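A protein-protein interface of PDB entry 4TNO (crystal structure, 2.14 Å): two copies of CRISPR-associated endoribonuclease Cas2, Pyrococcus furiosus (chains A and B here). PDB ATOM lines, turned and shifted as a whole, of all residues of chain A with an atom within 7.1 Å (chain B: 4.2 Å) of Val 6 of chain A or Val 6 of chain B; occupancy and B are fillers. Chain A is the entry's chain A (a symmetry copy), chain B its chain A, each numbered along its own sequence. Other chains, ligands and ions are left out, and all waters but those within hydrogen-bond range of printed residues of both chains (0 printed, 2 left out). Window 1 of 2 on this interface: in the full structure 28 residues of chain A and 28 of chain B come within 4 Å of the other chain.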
ATOM      1  N   VAL A   4      24.648  -9.627  15.217  1.00  0.00           N
ATOM      2  CA  VAL A   4      24.900 -11.049  15.015  1.00  0.00           C
ATOM      3  C   VAL A   4      25.076 -11.204  13.525  1.00  0.00           C
ATOM      4  O   VAL A   4      24.287 -10.706  12.711  1.00  0.00           O
ATOM      5  CB  VAL A   4      23.785 -12.008  15.550  1.00  0.00           C
ATOM      6  CG1 VAL A   4      23.457 -11.771  17.050  1.00  0.00           C
ATOM      7  CG2 VAL A   4      22.560 -11.938  14.721  1.00  0.00           C
ATOM      8  N   VAL A   5      26.170 -11.854  13.179  1.00  0.00           N
ATOM      9  CA  VAL A   5      26.571 -11.971  11.796  1.00  0.00           C
ATOM     10  C   VAL A   5      26.519 -13.435  11.435  1.00  0.00           C
ATOM     11  O   VAL A   5      27.178 -14.289  12.056  1.00  0.00           O
ATOM     12  CB  VAL A   5      27.965 -11.397  11.579  1.00  0.00           C
ATOM     13  CG1 VAL A   5      28.441 -11.700  10.165  1.00  0.00           C
ATOM     14  CG2 VAL A   5      27.966  -9.892  11.858  1.00  0.00           C
ATOM     15  N   VAL A   6      25.686 -13.754  10.468  1.00  0.00           N
ATOM     16  CA  VAL A   6      25.698 -15.121   9.985  1.00  0.00           C
ATOM     17  C   VAL A   6      25.904 -15.117   8.478  1.00  0.00           C
ATOM     18  O   VAL A   6      25.303 -14.330   7.755  1.00  0.00           O
ATOM     19  CB  VAL A   6      24.419 -15.881  10.398  1.00  0.00           C
ATOM     20  CG1 VAL A   6      23.181 -15.217   9.847  1.00  0.00           C
ATOM     21  CG2 VAL A   6      24.525 -17.352   9.954  1.00  0.00           C
ATOM     22  N   TYR A   7      26.795 -15.993   8.020  1.00  0.00           N
ATOM     23  CA  TYR A   7      27.219 -16.010   6.625  1.00  0.00           C
ATOM     24  C   TYR A   7      27.221 -17.409   6.010  1.00  0.00           C
ATOM     25  O   TYR A   7      27.443 -18.420   6.692  1.00  0.00           O
ATOM     26  CB  TYR A   7      28.624 -15.406   6.488  1.00  0.00           C
ATOM     27  CG  TYR A   7      29.673 -16.133   7.289  1.00  0.00           C
ATOM     28  CD1 TYR A   7      29.933 -15.784   8.616  1.00  0.00           C
ATOM     29  CD2 TYR A   7      30.410 -17.173   6.729  1.00  0.00           C
ATOM     30  CE1 TYR A   7      30.896 -16.457   9.368  1.00  0.00           C
ATOM     31  CE2 TYR A   7      31.375 -17.841   7.464  1.00  0.00           C
ATOM     32  CZ  TYR A   7      31.623 -17.472   8.781  1.00  0.00           C
ATOM     33  OH  TYR A   7      32.579 -18.142   9.516  1.00  0.00           O
ATOM     34  N   ASP A   8      26.974 -17.448   4.706  1.00  0.00           N
ATOM     35  CA  ASP A   8      27.145 -18.668   3.905  1.00  0.00           C
ATOM     36  C   ASP A   8      28.197 -18.394   2.830  1.00  0.00           C
ATOM     37  O   ASP A   8      27.899 -17.742   1.837  1.00  0.00           O
ATOM     38  CB  ASP A   8      25.811 -19.077   3.275  1.00  0.00           C
ATOM     39  CG  ASP A   8      25.903 -20.355   2.449  1.00  0.00           C
ATOM     40  OD1 ASP A   8      26.517 -21.355   2.896  1.00  0.00           O
ATOM     41  OD2 ASP A   8      25.322 -20.365   1.355  1.00  0.00           O
ATOM     42  N   LEU A  21      36.370 -11.875  11.015  1.00  0.00           N
ATOM     43  CA  LEU A  21      35.305 -11.619  11.982  1.00  0.00           C
ATOM     44  C   LEU A  21      35.826 -11.883  13.379  1.00  0.00           C
ATOM     45  O   LEU A  21      35.424 -11.230  14.328  1.00  0.00           O
ATOM     46  CB  LEU A  21      34.067 -12.477  11.689  1.00  0.00           C
ATOM     47  CG  LEU A  21      33.351 -12.126  10.388  1.00  0.00           C
ATOM     48  CD1 LEU A  21      32.104 -12.942  10.210  1.00  0.00           C
ATOM     49  CD2 LEU A  21      33.024 -10.635  10.348  1.00  0.00           C
ATOM     50  N   VAL A  28      30.435 -17.902  17.959  1.00  0.00           N
ATOM     51  CA  VAL A  28      29.582 -18.698  18.852  1.00  0.00           C
ATOM     52  C   VAL A  28      29.037 -19.994  18.259  1.00  0.00           C
ATOM     53  O   VAL A  28      28.571 -20.867  18.988  1.00  0.00           O
ATOM     54  CB  VAL A  28      28.392 -17.870  19.349  1.00  0.00           C
ATOM     55  CG1 VAL A  28      28.880 -16.787  20.291  1.00  0.00           C
ATOM     56  CG2 VAL A  28      27.631 -17.287  18.172  1.00  0.00           C
ATOM     57  N   GLN A  29      29.064 -20.105  16.938  1.00  0.00           N
ATOM     58  CA  GLN A  29      28.652 -21.321  16.249  1.00  0.00           C
ATOM     59  C   GLN A  29      29.305 -21.238  14.902  1.00  0.00           C
ATOM     60  O   GLN A  29      29.740 -20.156  14.498  1.00  0.00           O
ATOM     61  CB  GLN A  29      27.125 -21.426  16.117  1.00  0.00           C
ATOM     62  CG  GLN A  29      26.599 -22.754  15.551  1.00  0.00           C
ATOM     63  CD  GLN A  29      25.048 -22.851  15.557  1.00  0.00           C
ATOM     64  OE1 GLN A  29      24.441 -23.201  16.571  1.00  0.00           O
ATOM     65  NE2 GLN A  29      24.421 -22.547  14.419  1.00  0.00           N
ATOM     66  N   ASN A  30      29.405 -22.355  14.200  1.00  0.00           N
ATOM     67  CA  ASN A  30      29.907 -22.293  12.843  1.00  0.00           C
ATOM     68  C   ASN A  30      29.071 -21.345  11.977  1.00  0.00           C
ATOM     69  O   ASN A  30      27.843 -21.449  11.936  1.00  0.00           O
ATOM     70  CB  ASN A  30      29.923 -23.677  12.221  1.00  0.00           C
ATOM     71  CG  ASN A  30      30.408 -23.651  10.799  1.00  0.00           C
ATOM     72  OD1 ASN A  30      29.641 -23.339   9.881  1.00  0.00           O
ATOM     73  ND2 ASN A  30      31.696 -23.951  10.600  1.00  0.00           N
ATOM     74  N   SER A  31      29.757 -20.438  11.287  1.00  0.00           N
ATOM     75  CA  SER A  31      29.137 -19.412  10.460  1.00  0.00           C
ATOM     76  C   SER A  31      28.403 -18.314  11.249  1.00  0.00           C
ATOM     77  O   SER A  31      27.672 -17.572  10.645  1.00  0.00           O
ATOM     78  CB  SER A  31      28.123 -20.030   9.478  1.00  0.00           C
ATOM     79  OG  SER A  31      28.538 -21.299   9.011  1.00  0.00           O
ATOM     80  N   VAL A  32      28.561 -18.216  12.571  1.00  0.00           N
ATOM     81  CA  VAL A  32      27.840 -17.179  13.336  1.00  0.00           C
ATOM     82  C   VAL A  32      28.726 -16.403  14.314  1.00  0.00           C
ATOM     83  O   VAL A  32      29.395 -16.981  15.179  1.00  0.00           O
ATOM     84  CB  VAL A  32      26.674 -17.767  14.144  1.00  0.00           C
ATOM     85  CG1 VAL A  32      26.000 -16.652  14.995  1.00  0.00           C
ATOM     86  CG2 VAL A  32      25.681 -18.458  13.232  1.00  0.00           C
ATOM     87  N   PHE A  33      28.704 -15.082  14.178  1.00  0.00           N
ATOM     88  CA  PHE A  33      29.455 -14.205  15.063  1.00  0.00           C
ATOM     89  C   PHE A  33      28.581 -13.116  15.689  1.00  0.00           C
ATOM     90  O   PHE A  33      27.668 -12.600  15.048  1.00  0.00           O
ATOM     91  CB  PHE A  33      30.606 -13.510  14.308  1.00  0.00           C
ATOM     92  CG  PHE A  33      31.777 -14.418  13.976  1.00  0.00           C
ATOM     93  CD1 PHE A  33      31.718 -15.289  12.898  1.00  0.00           C
ATOM     94  CD2 PHE A  33      32.934 -14.377  14.729  1.00  0.00           C
ATOM     95  CE1 PHE A  33      32.792 -16.113  12.565  1.00  0.00           C
ATOM     96  CE2 PHE A  33      34.022 -15.199  14.403  1.00  0.00           C
ATOM     97  CZ  PHE A  33      33.944 -16.062  13.315  1.00  0.00           C
ATOM     98  N   SER A  59      26.418 -14.945   0.863  1.00  0.00           N
ATOM     99  CA  SER A  59      25.430 -14.191   1.642  1.00  0.00           C
ATOM    100  C   SER A  59      25.847 -13.900   3.089  1.00  0.00           C
ATOM    101  O   SER A  59      26.314 -14.779   3.810  1.00  0.00           O
ATOM    102  CB  SER A  59      24.102 -14.950   1.653  1.00  0.00           C
ATOM    103  OG  SER A  59      23.581 -15.071   0.339  1.00  0.00           O
ATOM    104  N   VAL A  60      25.656 -12.661   3.511  1.00  0.00           N
ATOM    105  CA  VAL A  60      25.863 -12.290   4.899  1.00  0.00           C
ATOM    106  C   VAL A  60      24.616 -11.581   5.377  1.00  0.00           C
ATOM    107  O   VAL A  60      24.144 -10.650   4.720  1.00  0.00           O
ATOM    108  CB  VAL A  60      27.083 -11.371   5.068  1.00  0.00           C
ATOM    109  CG1 VAL A  60      27.267 -10.961   6.515  1.00  0.00           C
ATOM    110  CG2 VAL A  60      28.303 -12.068   4.578  1.00  0.00           C
ATOM    111  N   ILE A  61      24.041 -12.052   6.478  1.00  0.00           N
ATOM    112  CA  ILE A  61      23.042 -11.265   7.162  1.00  0.00           C
ATOM    113  C   ILE A  61      23.683 -10.743   8.419  1.00  0.00           C
ATOM    114  O   ILE A  61      24.244 -11.497   9.222  1.00  0.00           O
ATOM    115  CB  ILE A  61      21.788 -12.047   7.525  1.00  0.00           C
ATOM    116  CG1 ILE A  61      21.141 -12.615   6.266  1.00  0.00           C
ATOM    117  CG2 ILE A  61      20.807 -11.140   8.260  1.00  0.00           C
ATOM    118  CD1 ILE A  61      19.921 -13.506   6.555  1.00  0.00           C
ATOM    119  N   ILE A  62      23.625  -9.433   8.565  1.00  0.00           N
ATOM    120  CA  ILE A  62      24.027  -8.804   9.803  1.00  0.00           C
ATOM    121  C   ILE A  62      22.804  -8.273  10.485  1.00  0.00           C
ATOM    122  O   ILE A  62      22.206  -7.304  10.032  1.00  0.00           O
ATOM    123  CB  ILE A  62      24.980  -7.666   9.584  1.00  0.00           C
ATOM    124  CG1 ILE A  62      26.118  -8.096   8.660  1.00  0.00           C
ATOM    125  CG2 ILE A  62      25.496  -7.177  10.924  1.00  0.00           C
ATOM    126  CD1 ILE A  62      27.119  -7.012   8.464  1.00  0.00           C
ATOM    127  N   TYR A  63      22.425  -8.892  11.577  1.00  0.00           N
ATOM    128  CA  TYR A  63      21.273  -8.387  12.270  1.00  0.00           C
ATOM    129  C   TYR A  63      21.735  -7.215  13.125  1.00  0.00           C
ATOM    130  O   TYR A  63      22.705  -7.338  13.871  1.00  0.00           O
ATOM    131  CB  TYR A  63      20.621  -9.467  13.118  1.00  0.00           C
ATOM    132  CG  TYR A  63      19.948 -10.614  12.353  1.00  0.00           C
ATOM    133  CD1 TYR A  63      18.627 -10.514  11.914  1.00  0.00           C
ATOM    134  CD2 TYR A  63      20.623 -11.814  12.110  1.00  0.00           C
ATOM    135  CE1 TYR A  63      18.005 -11.568  11.230  1.00  0.00           C
ATOM    136  CE2 TYR A  63      20.012 -12.863  11.438  1.00  0.00           C
ATOM    137  CZ  TYR A  63      18.715 -12.738  11.002  1.00  0.00           C
ATOM    138  OH  TYR A  63      18.142 -13.781  10.353  1.00  0.00           O
ATOM    139  N   VAL B   4      15.291 -15.786  15.767  1.00  0.00           N
ATOM    140  CA  VAL B   4      16.143 -16.159  14.643  1.00  0.00           C
ATOM    141  C   VAL B   4      16.839 -17.421  15.087  1.00  0.00           C
ATOM    142  O   VAL B   4      17.383 -17.523  16.194  1.00  0.00           O
ATOM    143  CB  VAL B   4      17.180 -15.073  14.202  1.00  0.00           C
ATOM    144  CG1 VAL B   4      16.519 -13.702  13.890  1.00  0.00           C
ATOM    145  CG2 VAL B   4      18.270 -14.924  15.193  1.00  0.00           C
ATOM    146  N   VAL B   5      16.753 -18.413  14.220  1.00  0.00           N
ATOM    147  CA  VAL B   5      17.237 -19.735  14.540  1.00  0.00           C
ATOM    148  C   VAL B   5      18.376 -20.038  13.596  1.00  0.00           C
ATOM    149  O   VAL B   5      18.228 -20.017  12.361  1.00  0.00           O
ATOM    150  CB  VAL B   5      16.127 -20.771  14.416  1.00  0.00           C
ATOM    151  CG1 VAL B   5      16.700 -22.173  14.571  1.00  0.00           C
ATOM    152  CG2 VAL B   5      15.033 -20.498  15.451  1.00  0.00           C
ATOM    153  N   VAL B   6      19.542 -20.261  14.163  1.00  0.00           N
ATOM    154  CA  VAL B   6      20.636 -20.694  13.317  1.00  0.00           C
ATOM    155  C   VAL B   6      21.220 -21.983  13.874  1.00  0.00           C
ATOM    156  O   VAL B   6      21.424 -22.122  15.076  1.00  0.00           O
ATOM    157  CB  VAL B   6      21.704 -19.590  13.158  1.00  0.00           C
ATOM    158  CG1 VAL B   6      22.291 -19.195  14.491  1.00  0.00           C
ATOM    159  CG2 VAL B   6      22.789 -20.057  12.170  1.00  0.00           C
ATOM    160  N   TYR B   7      21.456 -22.939  12.980  1.00  0.00           N
ATOM    161  CA  TYR B   7      21.868 -24.282  13.370  1.00  0.00           C
ATOM    162  C   TYR B   7      23.051 -24.811  12.560  1.00  0.00           C
ATOM    163  O   TYR B   7      23.241 -24.469  11.384  1.00  0.00           O
ATOM    164  CB  TYR B   7      20.694 -25.261  13.229  1.00  0.00           C
ATOM    165  CG  TYR B   7      20.144 -25.345  11.829  1.00  0.00           C
ATOM    166  CD1 TYR B   7      19.136 -24.478  11.400  1.00  0.00           C
ATOM    167  CD2 TYR B   7      20.625 -26.288  10.925  1.00  0.00           C
ATOM    168  CE1 TYR B   7      18.626 -24.544  10.104  1.00  0.00           C
ATOM    169  CE2 TYR B   7      20.119 -26.367   9.638  1.00  0.00           C
ATOM    170  CZ  TYR B   7      19.112 -25.499   9.235  1.00  0.00           C
ATOM    171  OH  TYR B   7      18.613 -25.572   7.950  1.00  0.00           O
ATOM    172  N   GLN B  29      18.497 -17.703   4.891  1.00  0.00           N
ATOM    173  CA  GLN B  29      19.849 -18.018   4.450  1.00  0.00           C
ATOM    174  C   GLN B  29      20.036 -19.466   4.788  1.00  0.00           C
ATOM    175  O   GLN B  29      19.270 -20.012   5.588  1.00  0.00           O
ATOM    176  CB  GLN B  29      20.906 -17.147   5.147  1.00  0.00           C
ATOM    177  CG  GLN B  29      22.341 -17.299   4.621  1.00  0.00           C
ATOM    178  CD  GLN B  29      23.342 -16.306   5.276  1.00  0.00           C
ATOM    179  OE1 GLN B  29      23.455 -15.153   4.855  1.00  0.00           O
ATOM    180  NE2 GLN B  29      24.064 -16.767   6.298  1.00  0.00           N
ATOM    181  N   SER B  31      20.957 -22.499   6.753  1.00  0.00           N
ATOM    182  CA  SER B  31      21.067 -22.698   8.192  1.00  0.00           C
ATOM    183  C   SER B  31      20.438 -21.579   9.040  1.00  0.00           C
ATOM    184  O   SER B  31      20.694 -21.546  10.217  1.00  0.00           O
ATOM    185  CB  SER B  31      22.542 -22.828   8.621  1.00  0.00           C
ATOM    186  OG  SER B  31      23.322 -23.502   7.652  1.00  0.00           O
ATOM    187  N   VAL B  32      19.656 -20.661   8.469  1.00  0.00           N
ATOM    188  CA  VAL B  32      19.069 -19.571   9.274  1.00  0.00           C
ATOM    189  C   VAL B  32      17.574 -19.355   9.029  1.00  0.00           C
ATOM    190  O   VAL B  32      17.129 -19.142   7.894  1.00  0.00           O
ATOM    191  CB  VAL B  32      19.771 -18.229   9.024  1.00  0.00           C
ATOM    192  CG1 VAL B  32      19.067 -17.100   9.830  1.00  0.00           C
ATOM    193  CG2 VAL B  32      21.247 -18.322   9.357  1.00  0.00           C
ATOM    194  N   SER B  59      24.394 -28.152  17.060  1.00  0.00           N
ATOM    195  CA  SER B  59      24.144 -26.893  17.768  1.00  0.00           C
ATOM    196  C   SER B  59      23.021 -26.037  17.168  1.00  0.00           C
ATOM    197  O   SER B  59      22.960 -25.816  15.961  1.00  0.00           O
ATOM    198  CB  SER B  59      25.430 -26.065  17.808  1.00  0.00           C
ATOM    199  OG  SER B  59      26.444 -26.746  18.529  1.00  0.00           O
ATOM    200  N   VAL B  60      22.147 -25.541  18.027  1.00  0.00           N
ATOM    201  CA  VAL B  60      21.128 -24.593  17.614  1.00  0.00           C
ATOM    202  C   VAL B  60      21.206 -23.400  18.540  1.00  0.00           C
ATOM    203  O   VAL B  60      21.208 -23.567  19.763  1.00  0.00           O
ATOM    204  CB  VAL B  60      19.720 -25.207  17.670  1.00  0.00           C
ATOM    205  CG1 VAL B  60      18.663 -24.197  17.272  1.00  0.00           C
ATOM    206  CG2 VAL B  60      19.657 -26.390  16.771  1.00  0.00           C
ATOM    207  N   ILE B  61      21.336 -22.206  17.973  1.00  0.00           N
ATOM    208  CA  ILE B  61      21.116 -21.010  18.754  1.00  0.00           C
ATOM    209  C   ILE B  61      19.800 -20.434  18.308  1.00  0.00           C
ATOM    210  O   ILE B  61      19.563 -20.206  17.117  1.00  0.00           O
ATOM    211  CB  ILE B  61      22.206 -19.961  18.588  1.00  0.00           C
ATOM    212  CG1 ILE B  61      23.556 -20.537  19.003  1.00  0.00           C
ATOM    213  CG2 ILE B  61      21.875 -18.733  19.430  1.00  0.00           C
ATOM    214  CD1 ILE B  61      24.730 -19.571  18.769  1.00  0.00           C
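The backbone NH (N) of Tyr 7 of chain B sits at hydrogen-bond distance from the backbone carbonyl oxygen (O) of Ser 31 of chain B (3.2 Å). N of Tyr 63 of chain A is in hydrogen-bond range of O of Val 4 of chain A, 2.8 Å away. O of Val 6 of chain B lies within hydrogen-bond range of N of Ile 61 of chain B (2.9 Å). N of Asp 8 of chain A is in hydrogen-bond range of O of Ser 59 of chain A (2.9 Å). O of Val 6 of chain A lies within hydrogen-bond range of N of Ile 61 of chain A. The backbone NH (N) of Tyr 7 of chain A is in hydrogen-bond range of the backbone carbonyl oxygen (O) of Ser 31 of chain A (3.2 Å).
Val 6 of chain A touches Gln 29 of chain B, and with the chains exchanged Gln 29 of chain A touches Val 6 of chain B. Tyr 7 of chain A touches Gln 29 of chain B, and with the chains exchanged Gln 29 of chain A touches Tyr 7 of chain B. Gln 29 of chain A touches Ser 59 of chain B, and with the chains exchanged Ser 59 of chain A touches Gln 29 of chain B. Gln 29 of chain A touches Val 60 of chain B, and with the chains exchanged Val 60 of chain A touches Gln 29 of chain B. Of the 17 pairs that touch across the chains among the printed residues, 13 have their exchanged pair printed and touching as well.
Of chain B, only Val 6, Gln 29 and Val 32 come within 4 Å of Val 6 of chain A. Printed residues of chain B within 4 Å of Val 28 of chain A: Ile 61 (3.7 Å). Of the printed residues of chain B, Gln 29 of chain A touches Val 6 (3.1 Å), Tyr 7 (3.2 Å), Ser 59 (3.1 Å), Val 60 (3.6 Å) and Ile 61 (3.5 Å). Printed residues of chain B within 4 Å of Val 32 of chain A: Val 6 (3.5 Å). Of the printed residues of chain B, Val 60 of chain A touches Gln 29. Of chain A, only Val 6 (3.9 Å), Gln 29 (3.1 Å) and Val 32 (3.5 Å) come within 4 Å of Val 6 of chain B. The nearest printed residue of chain B that does not touch Val 6 of chain A is Ser 31 of chain B (5.7 Å). The nearest residue of chain A that does not touch Val 6 of chain B is Asn 30 of chain A (5.2 Å). The nearest printed residue of chain B that does not touch Val 28 of chain A is Ser 59 of chain B (6.2 Å).
The backbone carbonyl oxygen of Ser 59 of chain B sits close to the side-chain amide oxygen of Gln 29 of chain A. The side-chain amide nitrogen (NE2) of Gln 29 of chain A is in hydrogen-bond range of the backbone carbonyl oxygen (O) of Val 6 of chain B (3.1 Å). The side-chain amide nitrogen (NE2) of Gln 29 of chain B sits close to the backbone NH (N) of Asp 8 of chain A, 3.4 Å away. N of Tyr 7 of chain B sits close to NE2 of Gln 29 of chain A, 3.3 Å away. NE2 of Gln 29 of chain B lies close to N of Tyr 7 of chain A (3.3 Å). NE2 of Gln 29 of chain B is in hydrogen-bond range of O of Val 6 of chain A, 3.1 Å away. The side-chain amide oxygen (OE1) of Gln 29 of chain B sits close to the backbone carbonyl oxygen (O) of Ser 59 of chain A (3.1 Å).
Printed residues of chain A that touch a printed residue of chain B: Val 6, Tyr 7, Asp 8, Val 28, Gln 29, Val 32, Ser 59, Val 60, Ile 61 and Tyr 63. Of the 10 printed residues of chain B, 8 touch a printed residue of chain A. Hydrophobic or aromatic side chains of chain B that line the printed part of chain A: Val 4, Val 6, Val 32 and Ile 61.
Among the printed residues, merely in contact across the chains: Val 6 of chain A with Val 32 of chain B (3.5 Å), Val 32 of chain A with Val 6 of chain B (3.5 Å), Tyr 63 of chain A with Val 32 of chain B (3.5 Å), Ile 61 of chain A with Gln 29 of chain B (3.5 Å), Gln 29 of chain A with Ile 61 of chain B (3.5 Å), Gln 29 of chain A with Val 60 of chain B (3.6 Å), Val 60 of chain A with Gln 29 of chain B (3.6 Å), Tyr 63 of chain A with Val 4 of chain B (3.7 Å), Val 28 of chain A with Ile 61 of chain B (3.7 Å) and Val 6 of chain A with Val 6 of chain B (3.9 Å).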
